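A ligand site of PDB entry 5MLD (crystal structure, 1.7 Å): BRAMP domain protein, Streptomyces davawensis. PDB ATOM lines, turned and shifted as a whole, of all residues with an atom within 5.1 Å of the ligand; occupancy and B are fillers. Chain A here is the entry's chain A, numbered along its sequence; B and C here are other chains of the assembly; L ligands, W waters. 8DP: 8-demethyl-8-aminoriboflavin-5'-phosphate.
The backbone NH (N) of Thr 21 sits at hydrogen-bond distance from the side-chain hydroxyl (OG) of Ser 19 (3.3 Å).
OG of Ser 19 lies within hydrogen-bond range of N of Gln 22, at 3.1 Å.
ND2 of Asn 9 lies within hydrogen-bond range of OG of Ser 19 (3.4 Å).
OD1 of Asn 9 lies within hydrogen-bond range of N of Thr 11 (2.9 Å).
The side-chain hydroxyl of Tyr 240 of chain B is in hydrogen-bond range of the side-chain carboxylate of Glu 135, 2.6 Å away.
N of Ile 91 sits at hydrogen-bond distance from O of Cys 132, 3.0 Å away.
The side-chain carboxylate (OD2) of Asp 136 is in hydrogen-bond range of the side-chain amide nitrogen (ND2) of Asn 94, at 3.5 Å.
OE2 of Glu 105 of chain C sits at hydrogen-bond distance from OG1 of Thr 92.
O1 of the ligand lies within hydrogen-bond range of OG of Ser 19, at 2.5 Å.
The side-chain hydroxyl (OG1) of Thr 11 lies within hydrogen-bond range of an oxygen (O3) of the ligand (2.6 Å).
The backbone NH of Glu 135 lies within hydrogen-bond range of an oxygen (O9) of the ligand (2.7 Å).
The backbone NH (N) of Ile 91 sits at hydrogen-bond distance from an oxygen (O7) of the ligand.
An oxygen (O7) of the ligand lies close to the backbone carbonyl oxygen of Ile 91, 2.7 Å away.
The backbone NH (N) of Asp 136 lies within hydrogen-bond range of an oxygen (O9) of the ligand, 2.7 Å away.
O of Asp 136 lies within hydrogen-bond range of N5 of the ligand.
N of Gln 20 lies within hydrogen-bond range of O2 of the ligand, 2.8 Å away.
The backbone NH (N) of Thr 21 lies within hydrogen-bond range of an oxygen (O1) of the ligand (3.0 Å).
OG1 of Thr 21 sits at hydrogen-bond distance from O1 of the ligand.
An oxygen (O8) of the ligand lies within hydrogen-bond range of the backbone NH (N) of Asn 94 (2.9 Å).
An oxygen (O9) of the ligand is in hydrogen-bond range of the backbone NH (N) of Asn 134 (2.9 Å).
O3 of the ligand is in salt-bridge range of NH2 of Arg 13 (3.0 Å).
O of Cys 132 is in hydrogen-bond range of O5 of the ligand, 3.1 Å away.
N of Leu 93 sits at hydrogen-bond distance from N3 of the ligand.
Water W3 lies within hydrogen-bond range of O6 of the ligand (2.5 Å), N of Arg 242 of chain B (3.2 Å) and ND2 of Asn 134 (3.3 Å).
Water W5 lies within hydrogen-bond range of an oxygen (O3) of the ligand (2.7 Å), the backbone NH of Leu 12 (3.0 Å) and the side-chain hydroxyl of Thr 11 (3.5 Å).
Water W6 bridges O of Tyr 240 of chain B (3.0 Å) and N2 of the ligand (3.1 Å).
Water W2 lies within hydrogen-bond range of OD1 of Asn 134 (3.0 Å), O5 of the ligand (3.1 Å) and SG of Cys 132 (3.3 Å).
Water W4 bridges O6 of the ligand (3.1 Å) and NH2 of Arg 13 (3.4 Å).
Residues that only touch the ligand: Pro 90 (3.5 Å), Thr 92 (3.4 Å), Gly 133 (3.4 Å), Tyr 240 of chain B (3.3 Å), Glu 105 of chain C (3.6 Å), Asn 108 of chain C (3.9 Å) and Leu 109 of chain C (3.8 Å).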
ATOM      1  N   ASN A   9     -17.747  37.863  10.428  1.00  0.00           N
ATOM      2  CA  ASN A   9     -18.780  37.301   9.565  1.00  0.00           C
ATOM      3  C   ASN A   9     -18.196  37.180   8.167  1.00  0.00           C
ATOM      4  O   ASN A   9     -17.921  38.189   7.511  1.00  0.00           O
ATOM      5  CB  ASN A   9     -20.042  38.176   9.557  1.00  0.00           C
ATOM      6  CG  ASN A   9     -21.157  37.534   8.785  1.00  0.00           C
ATOM      7  OD1 ASN A   9     -20.915  36.670   7.955  1.00  0.00           O
ATOM      8  ND2 ASN A   9     -22.384  37.946   9.069  1.00  0.00           N
ATOM      9  N   THR A  11     -19.621  35.883   5.435  1.00  0.00           N
ATOM     10  CA  THR A  11     -20.599  35.806   4.352  1.00  0.00           C
ATOM     11  C   THR A  11     -20.092  36.501   3.093  1.00  0.00           C
ATOM     12  O   THR A  11     -19.288  37.439   3.155  1.00  0.00           O
ATOM     13  CB  THR A  11     -21.923  36.456   4.781  1.00  0.00           C
ATOM     14  OG1 THR A  11     -22.867  36.363   3.716  1.00  0.00           O
ATOM     15  CG2 THR A  11     -21.717  37.932   5.138  1.00  0.00           C
ATOM     16  N   LEU A  12     -20.579  36.050   1.940  1.00  0.00           N
ATOM     17  CA  LEU A  12     -20.190  36.617   0.664  1.00  0.00           C
ATOM     18  C   LEU A  12     -21.065  37.787   0.217  1.00  0.00           C
ATOM     19  O   LEU A  12     -20.772  38.382  -0.821  1.00  0.00           O
ATOM     20  CB  LEU A  12     -20.216  35.530  -0.419  1.00  0.00           C
ATOM     21  CG  LEU A  12     -19.190  34.445  -0.155  1.00  0.00           C
ATOM     22  CD1 LEU A  12     -19.294  33.359  -1.232  1.00  0.00           C
ATOM     23  CD2 LEU A  12     -17.778  35.018  -0.108  1.00  0.00           C
ATOM     24  N   ARG A  13     -22.106  38.120   0.971  1.00  0.00           N
ATOM     25  CA  ARG A  13     -22.977  39.234   0.582  1.00  0.00           C
ATOM     26  C   ARG A  13     -22.585  40.488   1.366  1.00  0.00           C
ATOM     27  O   ARG A  13     -22.435  40.453   2.588  1.00  0.00           O
ATOM     28  CB  ARG A  13     -24.449  38.864   0.803  1.00  0.00           C
ATOM     29  CG  ARG A  13     -24.895  38.744   2.256  1.00  0.00           C
ATOM     30  CD  ARG A  13     -26.179  37.941   2.363  1.00  0.00           C
ATOM     31  NE  ARG A  13     -25.919  36.522   2.225  1.00  0.00           N
ATOM     32  CZ  ARG A  13     -26.186  35.774   1.154  1.00  0.00           C
ATOM     33  NH1 ARG A  13     -26.751  36.318   0.078  1.00  0.00           N
ATOM     34  NH2 ARG A  13     -25.874  34.487   1.166  1.00  0.00           N
ATOM     35  N   ARG A  18     -29.104  40.854   4.099  1.00  0.00           N
ATOM     36  CA  ARG A  18     -29.381  40.052   5.263  1.00  0.00           C
ATOM     37  C   ARG A  18     -28.613  38.730   5.200  1.00  0.00           C
ATOM     38  O   ARG A  18     -28.669  38.030   4.187  1.00  0.00           O
ATOM     39  CB  ARG A  18     -30.889  39.807   5.387  1.00  0.00           C
ATOM     40  CG  ARG A  18     -31.282  39.247   6.741  1.00  0.00           C
ATOM     41  CD  ARG A  18     -32.802  39.256   6.909  1.00  0.00           C
ATOM     42  NE  ARG A  18     -33.521  38.951   5.674  1.00  0.00           N
ATOM     43  CZ  ARG A  18     -34.808  38.601   5.609  1.00  0.00           C
ATOM     44  NH1 ARG A  18     -35.521  38.484   6.717  1.00  0.00           N
ATOM     45  NH2 ARG A  18     -35.378  38.355   4.430  1.00  0.00           N
ATOM     46  N   SER A  19     -27.903  38.407   6.269  1.00  0.00           N
ATOM     47  CA  SER A  19     -27.069  37.216   6.355  1.00  0.00           C
ATOM     48  C   SER A  19     -27.675  36.210   7.331  1.00  0.00           C
ATOM     49  O   SER A  19     -28.019  36.583   8.461  1.00  0.00           O
ATOM     50  CB  SER A  19     -25.633  37.597   6.766  1.00  0.00           C
ATOM     51  OG  SER A  19     -24.921  36.523   7.391  1.00  0.00           O
ATOM     52  N   GLN A  20     -27.794  34.947   6.894  1.00  0.00           N
ATOM     53  CA  GLN A  20     -28.231  33.873   7.792  1.00  0.00           C
ATOM     54  C   GLN A  20     -27.281  33.736   8.985  1.00  0.00           C
ATOM     55  O   GLN A  20     -27.731  33.600  10.130  1.00  0.00           O
ATOM     56  CB  GLN A  20     -28.304  32.526   7.025  1.00  0.00           C
ATOM     57  CG  GLN A  20     -29.000  32.548   5.646  1.00  0.00           C
ATOM     58  CD  GLN A  20     -30.485  32.844   5.717  1.00  0.00           C
ATOM     59  OE1 GLN A  20     -31.228  32.173   6.440  1.00  0.00           O
ATOM     60  NE2 GLN A  20     -30.923  33.851   4.958  1.00  0.00           N
ATOM     61  N   THR A  21     -25.975  33.746   8.717  1.00  0.00           N
ATOM     62  CA  THR A  21     -24.980  33.540   9.749  1.00  0.00           C
ATOM     63  C   THR A  21     -25.047  34.625  10.806  1.00  0.00           C
ATOM     64  O   THR A  21     -24.788  34.374  11.986  1.00  0.00           O
ATOM     65  CB  THR A  21     -23.567  33.521   9.137  1.00  0.00           C
ATOM     66  OG1 THR A  21     -23.549  32.629   8.024  1.00  0.00           O
ATOM     67  CG2 THR A  21     -22.544  33.047  10.155  1.00  0.00           C
ATOM     68  N   GLN A  22     -25.398  35.853  10.386  1.00  0.00           N
ATOM     69  CA  GLN A  22     -25.495  36.978  11.314  1.00  0.00           C
ATOM     70  C   GLN A  22     -26.455  36.676  12.463  1.00  0.00           C
ATOM     71  O   GLN A  22     -26.303  37.229  13.558  1.00  0.00           O
ATOM     72  CB  GLN A  22     -25.927  38.228  10.546  1.00  0.00           C
ATOM     73  CG  GLN A  22     -25.941  39.513  11.393  1.00  0.00           C
ATOM     74  CD  GLN A  22     -24.551  39.925  11.835  1.00  0.00           C
ATOM     75  OE1 GLN A  22     -23.564  39.686  11.135  1.00  0.00           O
ATOM     76  NE2 GLN A  22     -24.454  40.541  13.013  1.00  0.00           N
ATOM     77  N   PRO A  90     -20.675  31.093   6.916  1.00  0.00           N
ATOM     78  CA  PRO A  90     -21.541  30.185   6.170  1.00  0.00           C
ATOM     79  C   PRO A  90     -20.696  29.024   5.661  1.00  0.00           C
ATOM     80  O   PRO A  90     -19.456  29.095   5.607  1.00  0.00           O
ATOM     81  CB  PRO A  90     -22.054  31.037   5.006  1.00  0.00           C
ATOM     82  CG  PRO A  90     -21.631  32.435   5.288  1.00  0.00           C
ATOM     83  CD  PRO A  90     -20.469  32.378   6.227  1.00  0.00           C
ATOM     84  N   ILE A  91     -21.366  27.950   5.259  1.00  0.00           N
ATOM     85  CA  ILE A  91     -20.701  26.792   4.669  1.00  0.00           C
ATOM     86  C   ILE A  91     -20.873  26.846   3.155  1.00  0.00           C
ATOM     87  O   ILE A  91     -22.000  26.978   2.661  1.00  0.00           O
ATOM     88  CB  ILE A  91     -21.281  25.483   5.228  1.00  0.00           C
ATOM     89  CG1 ILE A  91     -21.023  25.439   6.740  1.00  0.00           C
ATOM     90  CG2 ILE A  91     -20.690  24.273   4.452  1.00  0.00           C
ATOM     91  CD1 ILE A  91     -21.784  24.360   7.503  1.00  0.00           C
ATOM     92  N   THR A  92     -19.756  26.738   2.422  1.00  0.00           N
ATOM     93  CA  THR A  92     -19.853  26.562   0.961  1.00  0.00           C
ATOM     94  C   THR A  92     -18.946  25.424   0.549  1.00  0.00           C
ATOM     95  O   THR A  92     -17.771  25.400   0.925  1.00  0.00           O
ATOM     96  CB  THR A  92     -19.511  27.830   0.152  1.00  0.00           C
ATOM     97  OG1 THR A  92     -18.137  28.224   0.336  1.00  0.00           O
ATOM     98  CG2 THR A  92     -20.447  28.987   0.483  1.00  0.00           C
ATOM     99  N   LEU A  93     -19.489  24.504  -0.264  1.00  0.00           N
ATOM    100  CA  LEU A  93     -18.757  23.347  -0.778  1.00  0.00           C
ATOM    101  C   LEU A  93     -18.189  22.487   0.351  1.00  0.00           C
ATOM    102  O   LEU A  93     -17.086  21.959   0.231  1.00  0.00           O
ATOM    103  CB  LEU A  93     -17.623  23.771  -1.711  1.00  0.00           C
ATOM    104  CG  LEU A  93     -17.885  24.981  -2.622  1.00  0.00           C
ATOM    105  CD1 LEU A  93     -16.592  25.415  -3.268  1.00  0.00           C
ATOM    106  CD2 LEU A  93     -18.940  24.646  -3.646  1.00  0.00           C
ATOM    107  N   ASN A  94     -18.913  22.393   1.470  1.00  0.00           N
ATOM    108  CA  ASN A  94     -18.466  21.673   2.664  1.00  0.00           C
ATOM    109  C   ASN A  94     -17.189  22.277   3.257  1.00  0.00           C
ATOM    110  O   ASN A  94     -16.431  21.567   3.936  1.00  0.00           O
ATOM    111  CB  ASN A  94     -18.237  20.185   2.372  1.00  0.00           C
ATOM    112  CG  ASN A  94     -18.961  19.286   3.374  1.00  0.00           C
ATOM    113  OD1 ASN A  94     -18.341  18.521   4.098  1.00  0.00           O
ATOM    114  ND2 ASN A  94     -20.263  19.406   3.421  1.00  0.00           N
ATOM    115  N   CYS A 132     -23.133  28.350   9.752  1.00  0.00           N
ATOM    116  CA  CYS A 132     -24.507  28.235   9.266  1.00  0.00           C
ATOM    117  C   CYS A 132     -24.473  27.549   7.908  1.00  0.00           C
ATOM    118  O   CYS A 132     -23.782  28.014   7.010  1.00  0.00           O
ATOM    119  CB  CYS A 132     -25.163  29.616   9.142  1.00  0.00           C
ATOM    120  SG  CYS A 132     -26.905  29.438   9.067  1.00  0.00           S
ATOM    121  N   GLY A 133     -25.195  26.435   7.759  1.00  0.00           N
ATOM    122  CA  GLY A 133     -25.339  25.806   6.475  1.00  0.00           C
ATOM    123  C   GLY A 133     -26.803  25.451   6.251  1.00  0.00           C
ATOM    124  O   GLY A 133     -27.591  25.426   7.191  1.00  0.00           O
ATOM    125  N   ASN A 134     -27.151  25.162   4.998  1.00  0.00           N
ATOM    126  CA  ASN A 134     -28.529  24.723   4.795  1.00  0.00           C
ATOM    127  C   ASN A 134     -28.762  23.287   5.250  1.00  0.00           C
ATOM    128  O   ASN A 134     -29.915  22.940   5.595  1.00  0.00           O
ATOM    129  CB  ASN A 134     -28.927  24.870   3.313  1.00  0.00           C
ATOM    130  CG  ASN A 134     -29.167  26.314   2.916  1.00  0.00           C
ATOM    131  OD1 ASN A 134     -29.064  27.229   3.756  1.00  0.00           O
ATOM    132  ND2 ASN A 134     -29.494  26.541   1.650  1.00  0.00           N
ATOM    133  N   GLU A 135     -27.717  22.443   5.247  1.00  0.00           N
ATOM    134  CA  GLU A 135     -27.939  21.034   5.532  1.00  0.00           C
ATOM    135  C   GLU A 135     -26.741  20.276   6.110  1.00  0.00           C
ATOM    136  O   GLU A 135     -26.945  19.325   6.854  1.00  0.00           O
ATOM    137  CB  GLU A 135     -28.390  20.285   4.265  1.00  0.00           C
ATOM    138  CG  GLU A 135     -27.405  20.369   3.118  1.00  0.00           C
ATOM    139  CD  GLU A 135     -27.456  19.189   2.165  1.00  0.00           C
ATOM    140  OE1 GLU A 135     -26.677  19.200   1.187  1.00  0.00           O
ATOM    141  OE2 GLU A 135     -28.252  18.240   2.381  1.00  0.00           O
ATOM    142  N   ASP A 136     -25.495  20.633   5.751  1.00  0.00           N
ATOM    143  CA  ASP A 136     -24.421  19.687   6.043  1.00  0.00           C
ATOM    144  C   ASP A 136     -23.054  20.359   5.963  1.00  0.00           C
ATOM    145  O   ASP A 136     -22.827  21.211   5.102  1.00  0.00           O
ATOM    146  CB  ASP A 136     -24.501  18.518   5.051  1.00  0.00           C
ATOM    147  CG  ASP A 136     -23.474  17.451   5.315  1.00  0.00           C
ATOM    148  OD1 ASP A 136     -23.431  16.925   6.447  1.00  0.00           O
ATOM    149  OD2 ASP A 136     -22.720  17.141   4.383  1.00  0.00           O
ATOM    150  N   GLY A 137     -22.143  19.954   6.866  1.00  0.00           N
ATOM    151  CA  GLY A 137     -20.756  20.371   6.752  1.00  0.00           C
ATOM    152  C   GLY A 137     -20.154  20.980   8.010  1.00  0.00           C
ATOM    153  O   GLY A 137     -18.968  21.313   8.036  1.00  0.00           O
ATOM    154  N   LEU A 165     -27.962  23.883  11.114  1.00  0.00           N
ATOM    155  CA  LEU A 165     -28.174  23.183   9.856  1.00  0.00           C
ATOM    156  C   LEU A 165     -29.625  22.740   9.814  1.00  0.00           C
ATOM    157  O   LEU A 165     -30.203  22.384  10.847  1.00  0.00           O
ATOM    158  CB  LEU A 165     -27.290  21.920   9.712  1.00  0.00           C
ATOM    159  CG  LEU A 165     -25.782  22.060   9.876  1.00  0.00           C
ATOM    160  CD1 LEU A 165     -25.246  20.629   9.935  1.00  0.00           C
ATOM    161  CD2 LEU A 165     -25.162  22.865   8.752  1.00  0.00           C
ATOM    162  N   TYR B 240     -28.429  25.114  -3.670  1.00  0.00           N
ATOM    163  CA  TYR B 240     -28.886  25.601  -2.367  1.00  0.00           C
ATOM    164  C   TYR B 240     -29.716  26.859  -2.506  1.00  0.00           C
ATOM    165  O   TYR B 240     -29.389  27.761  -3.289  1.00  0.00           O
ATOM    166  CB  TYR B 240     -27.698  25.868  -1.441  1.00  0.00           C
ATOM    167  CG  TYR B 240     -27.046  24.586  -1.036  1.00  0.00           C
ATOM    168  CD1 TYR B 240     -27.745  23.659  -0.278  1.00  0.00           C
ATOM    169  CD2 TYR B 240     -25.766  24.271  -1.467  1.00  0.00           C
ATOM    170  CE1 TYR B 240     -27.167  22.444   0.080  1.00  0.00           C
ATOM    171  CE2 TYR B 240     -25.187  23.080  -1.124  1.00  0.00           C
ATOM    172  CZ  TYR B 240     -25.883  22.181  -0.348  1.00  0.00           C
ATOM    173  OH  TYR B 240     -25.304  20.985  -0.014  1.00  0.00           O
ATOM    174  N   ARG B 242     -31.389  29.495   0.214  1.00  0.00           N
ATOM    175  CA  ARG B 242     -31.613  29.841   1.609  1.00  0.00           C
ATOM    176  C   ARG B 242     -32.988  30.453   1.865  1.00  0.00           C
ATOM    177  O   ARG B 242     -33.457  30.430   3.001  1.00  0.00           O
ATOM    178  CB  ARG B 242     -30.524  30.811   2.074  1.00  0.00           C
ATOM    179  CG  ARG B 242     -30.655  32.193   1.494  1.00  0.00           C
ATOM    180  CD  ARG B 242     -29.308  32.900   1.347  1.00  0.00           C
ATOM    181  NE  ARG B 242     -29.512  34.290   0.921  1.00  0.00           N
ATOM    182  CZ  ARG B 242     -29.819  34.658  -0.316  1.00  0.00           C
ATOM    183  NH1 ARG B 242     -29.961  33.755  -1.290  1.00  0.00           N
ATOM    184  NH2 ARG B 242     -30.005  35.939  -0.582  1.00  0.00           N
ATOM    185  N   TYR C  53     -21.555  38.012  -3.659  1.00  0.00           N
ATOM    186  CA  TYR C  53     -22.792  37.383  -4.087  1.00  0.00           C
ATOM    187  C   TYR C  53     -23.935  38.388  -4.021  1.00  0.00           C
ATOM    188  O   TYR C  53     -24.031  39.162  -3.065  1.00  0.00           O
ATOM    189  CB  TYR C  53     -23.128  36.162  -3.201  1.00  0.00           C
ATOM    190  CG  TYR C  53     -24.398  35.464  -3.583  1.00  0.00           C
ATOM    191  CD1 TYR C  53     -25.637  35.931  -3.144  1.00  0.00           C
ATOM    192  CD2 TYR C  53     -24.376  34.358  -4.423  1.00  0.00           C
ATOM    193  CE1 TYR C  53     -26.817  35.293  -3.500  1.00  0.00           C
ATOM    194  CE2 TYR C  53     -25.563  33.709  -4.784  1.00  0.00           C
ATOM    195  CZ  TYR C  53     -26.778  34.196  -4.323  1.00  0.00           C
ATOM    196  OH  TYR C  53     -27.949  33.569  -4.675  1.00  0.00           O
ATOM    197  N   GLU C 105     -17.550  28.049  -6.091  1.00  0.00           N
ATOM    198  CA  GLU C 105     -18.725  28.738  -5.558  1.00  0.00           C
ATOM    199  C   GLU C 105     -19.591  29.264  -6.692  1.00  0.00           C
ATOM    200  O   GLU C 105     -20.810  29.050  -6.717  1.00  0.00           O
ATOM    201  CB  GLU C 105     -18.309  29.882  -4.625  1.00  0.00           C
ATOM    202  CG  GLU C 105     -18.029  29.440  -3.187  1.00  0.00           C
ATOM    203  CD  GLU C 105     -17.378  30.541  -2.354  1.00  0.00           C
ATOM    204  OE1 GLU C 105     -16.989  31.605  -2.923  1.00  0.00           O
ATOM    205  OE2 GLU C 105     -17.235  30.338  -1.122  1.00  0.00           O
ATOM    206  N   ASN C 108     -21.312  26.609  -8.728  1.00  0.00           N
ATOM    207  CA  ASN C 108     -22.412  25.990  -7.997  1.00  0.00           C
ATOM    208  C   ASN C 108     -23.675  26.853  -7.998  1.00  0.00           C
ATOM    209  O   ASN C 108     -24.704  26.404  -7.483  1.00  0.00           O
ATOM    210  CB  ASN C 108     -21.981  25.669  -6.564  1.00  0.00           C
ATOM    211  CG  ASN C 108     -21.295  24.315  -6.447  1.00  0.00           C
ATOM    212  OD1 ASN C 108     -21.883  23.359  -5.951  1.00  0.00           O
ATOM    213  ND2 ASN C 108     -20.052  24.237  -6.903  1.00  0.00           N
ATOM    214  N   LEU C 109     -23.613  28.065  -8.549  1.00  0.00           N
ATOM    215  CA  LEU C 109     -24.747  28.967  -8.609  1.00  0.00           C
ATOM    216  C   LEU C 109     -25.599  28.767  -9.851  1.00  0.00           C
ATOM    217  O   LEU C 109     -26.627  29.438 -10.001  1.00  0.00           O
ATOM    218  CB  LEU C 109     -24.276  30.427  -8.558  1.00  0.00           C
ATOM    219  CG  LEU C 109     -23.590  30.829  -7.250  1.00  0.00           C
ATOM    220  CD1 LEU C 109     -23.184  32.300  -7.282  1.00  0.00           C
ATOM    221  CD2 LEU C 109     -24.521  30.516  -6.062  1.00  0.00           C
HETATM  222  C4  8DP L   1     -25.251  28.057   2.740  1.00  0.00           C
HETATM  223  C5  8DP L   1     -25.897  27.069   1.766  1.00  0.00           C
HETATM  224  C8  8DP L   1     -23.863  28.386  -1.745  1.00  0.00           C
HETATM  225  N3  8DP L   1     -22.639  24.835   0.043  1.00  0.00           N
HETATM  226  C2  8DP L   1     -26.218  30.121   3.952  1.00  0.00           C
HETATM  227  N2  8DP L   1     -24.230  29.607  -2.407  1.00  0.00           N
HETATM  228  N1  8DP L   1     -24.763  26.268   1.128  1.00  0.00           N
HETATM  229  C6  8DP L   1     -24.121  26.732   0.035  1.00  0.00           C
HETATM  230  O6  8DP L   1     -26.560  29.802   1.658  1.00  0.00           O
HETATM  231  N4  8DP L   1     -24.987  24.640   2.807  1.00  0.00           N
HETATM  232  C12 8DP L   1     -23.058  25.991  -0.527  1.00  0.00           C
HETATM  233  C13 8DP L   1     -24.352  25.106   1.702  1.00  0.00           C
HETATM  234  C14 8DP L   1     -23.278  24.398   1.154  1.00  0.00           C
HETATM  235  C15 8DP L   1     -22.902  23.207   1.797  1.00  0.00           C
HETATM  236  C16 8DP L   1     -24.593  23.516   3.372  1.00  0.00           C
HETATM  237  C1  8DP L   1     -26.061  31.637   3.819  1.00  0.00           C
HETATM  238  C3  8DP L   1     -25.626  29.551   2.664  1.00  0.00           C
HETATM  239  C7  8DP L   1     -24.546  27.927  -0.594  1.00  0.00           C
HETATM  240  C9  8DP L   1     -22.780  27.618  -2.282  1.00  0.00           C
HETATM  241  O1  8DP L   1     -24.619  34.428   6.100  1.00  0.00           O
HETATM  242  P1  8DP L   1     -25.157  33.847   4.773  1.00  0.00           P
HETATM  243  O2  8DP L   1     -26.564  34.467   4.474  1.00  0.00           O
HETATM  244  O3  8DP L   1     -24.201  34.109   3.614  1.00  0.00           O
HETATM  245  O4  8DP L   1     -25.362  32.256   4.968  1.00  0.00           O
HETATM  246  O5  8DP L   1     -25.590  29.706   5.120  1.00  0.00           O
HETATM  247  O7  8DP L   1     -24.408  27.707   3.591  1.00  0.00           O
HETATM  248  C10 8DP L   1     -22.043  28.089  -3.516  1.00  0.00           C
HETATM  249  C11 8DP L   1     -22.389  26.457  -1.670  1.00  0.00           C
HETATM  250  O8  8DP L   1     -21.824  22.447   1.315  1.00  0.00           O
HETATM  251  N5  8DP L   1     -23.562  22.796   2.881  1.00  0.00           N
HETATM  252  O9  8DP L   1     -25.223  23.006   4.527  1.00  0.00           O
HETATM  253  O   HOH W   1     -22.849  32.322  -1.356  1.00  0.00           O
HETATM  254  O   HOH W   2     -28.415  28.966   6.165  1.00  0.00           O
HETATM  255  O   HOH W   3     -28.192  29.049  -0.085  1.00  0.00           O
HETATM  256  O   HOH W   4     -24.187  31.596   0.627  1.00  0.00           O
HETATM  257  O   HOH W   5     -22.176  33.506   1.908  1.00  0.00           O
HETATM  258  O   HOH W   6     -26.548  28.398  -3.988  1.00  0.00           O
HETATM  259  O   HOH W   7     -28.765  35.366   3.469  1.00  0.00           O
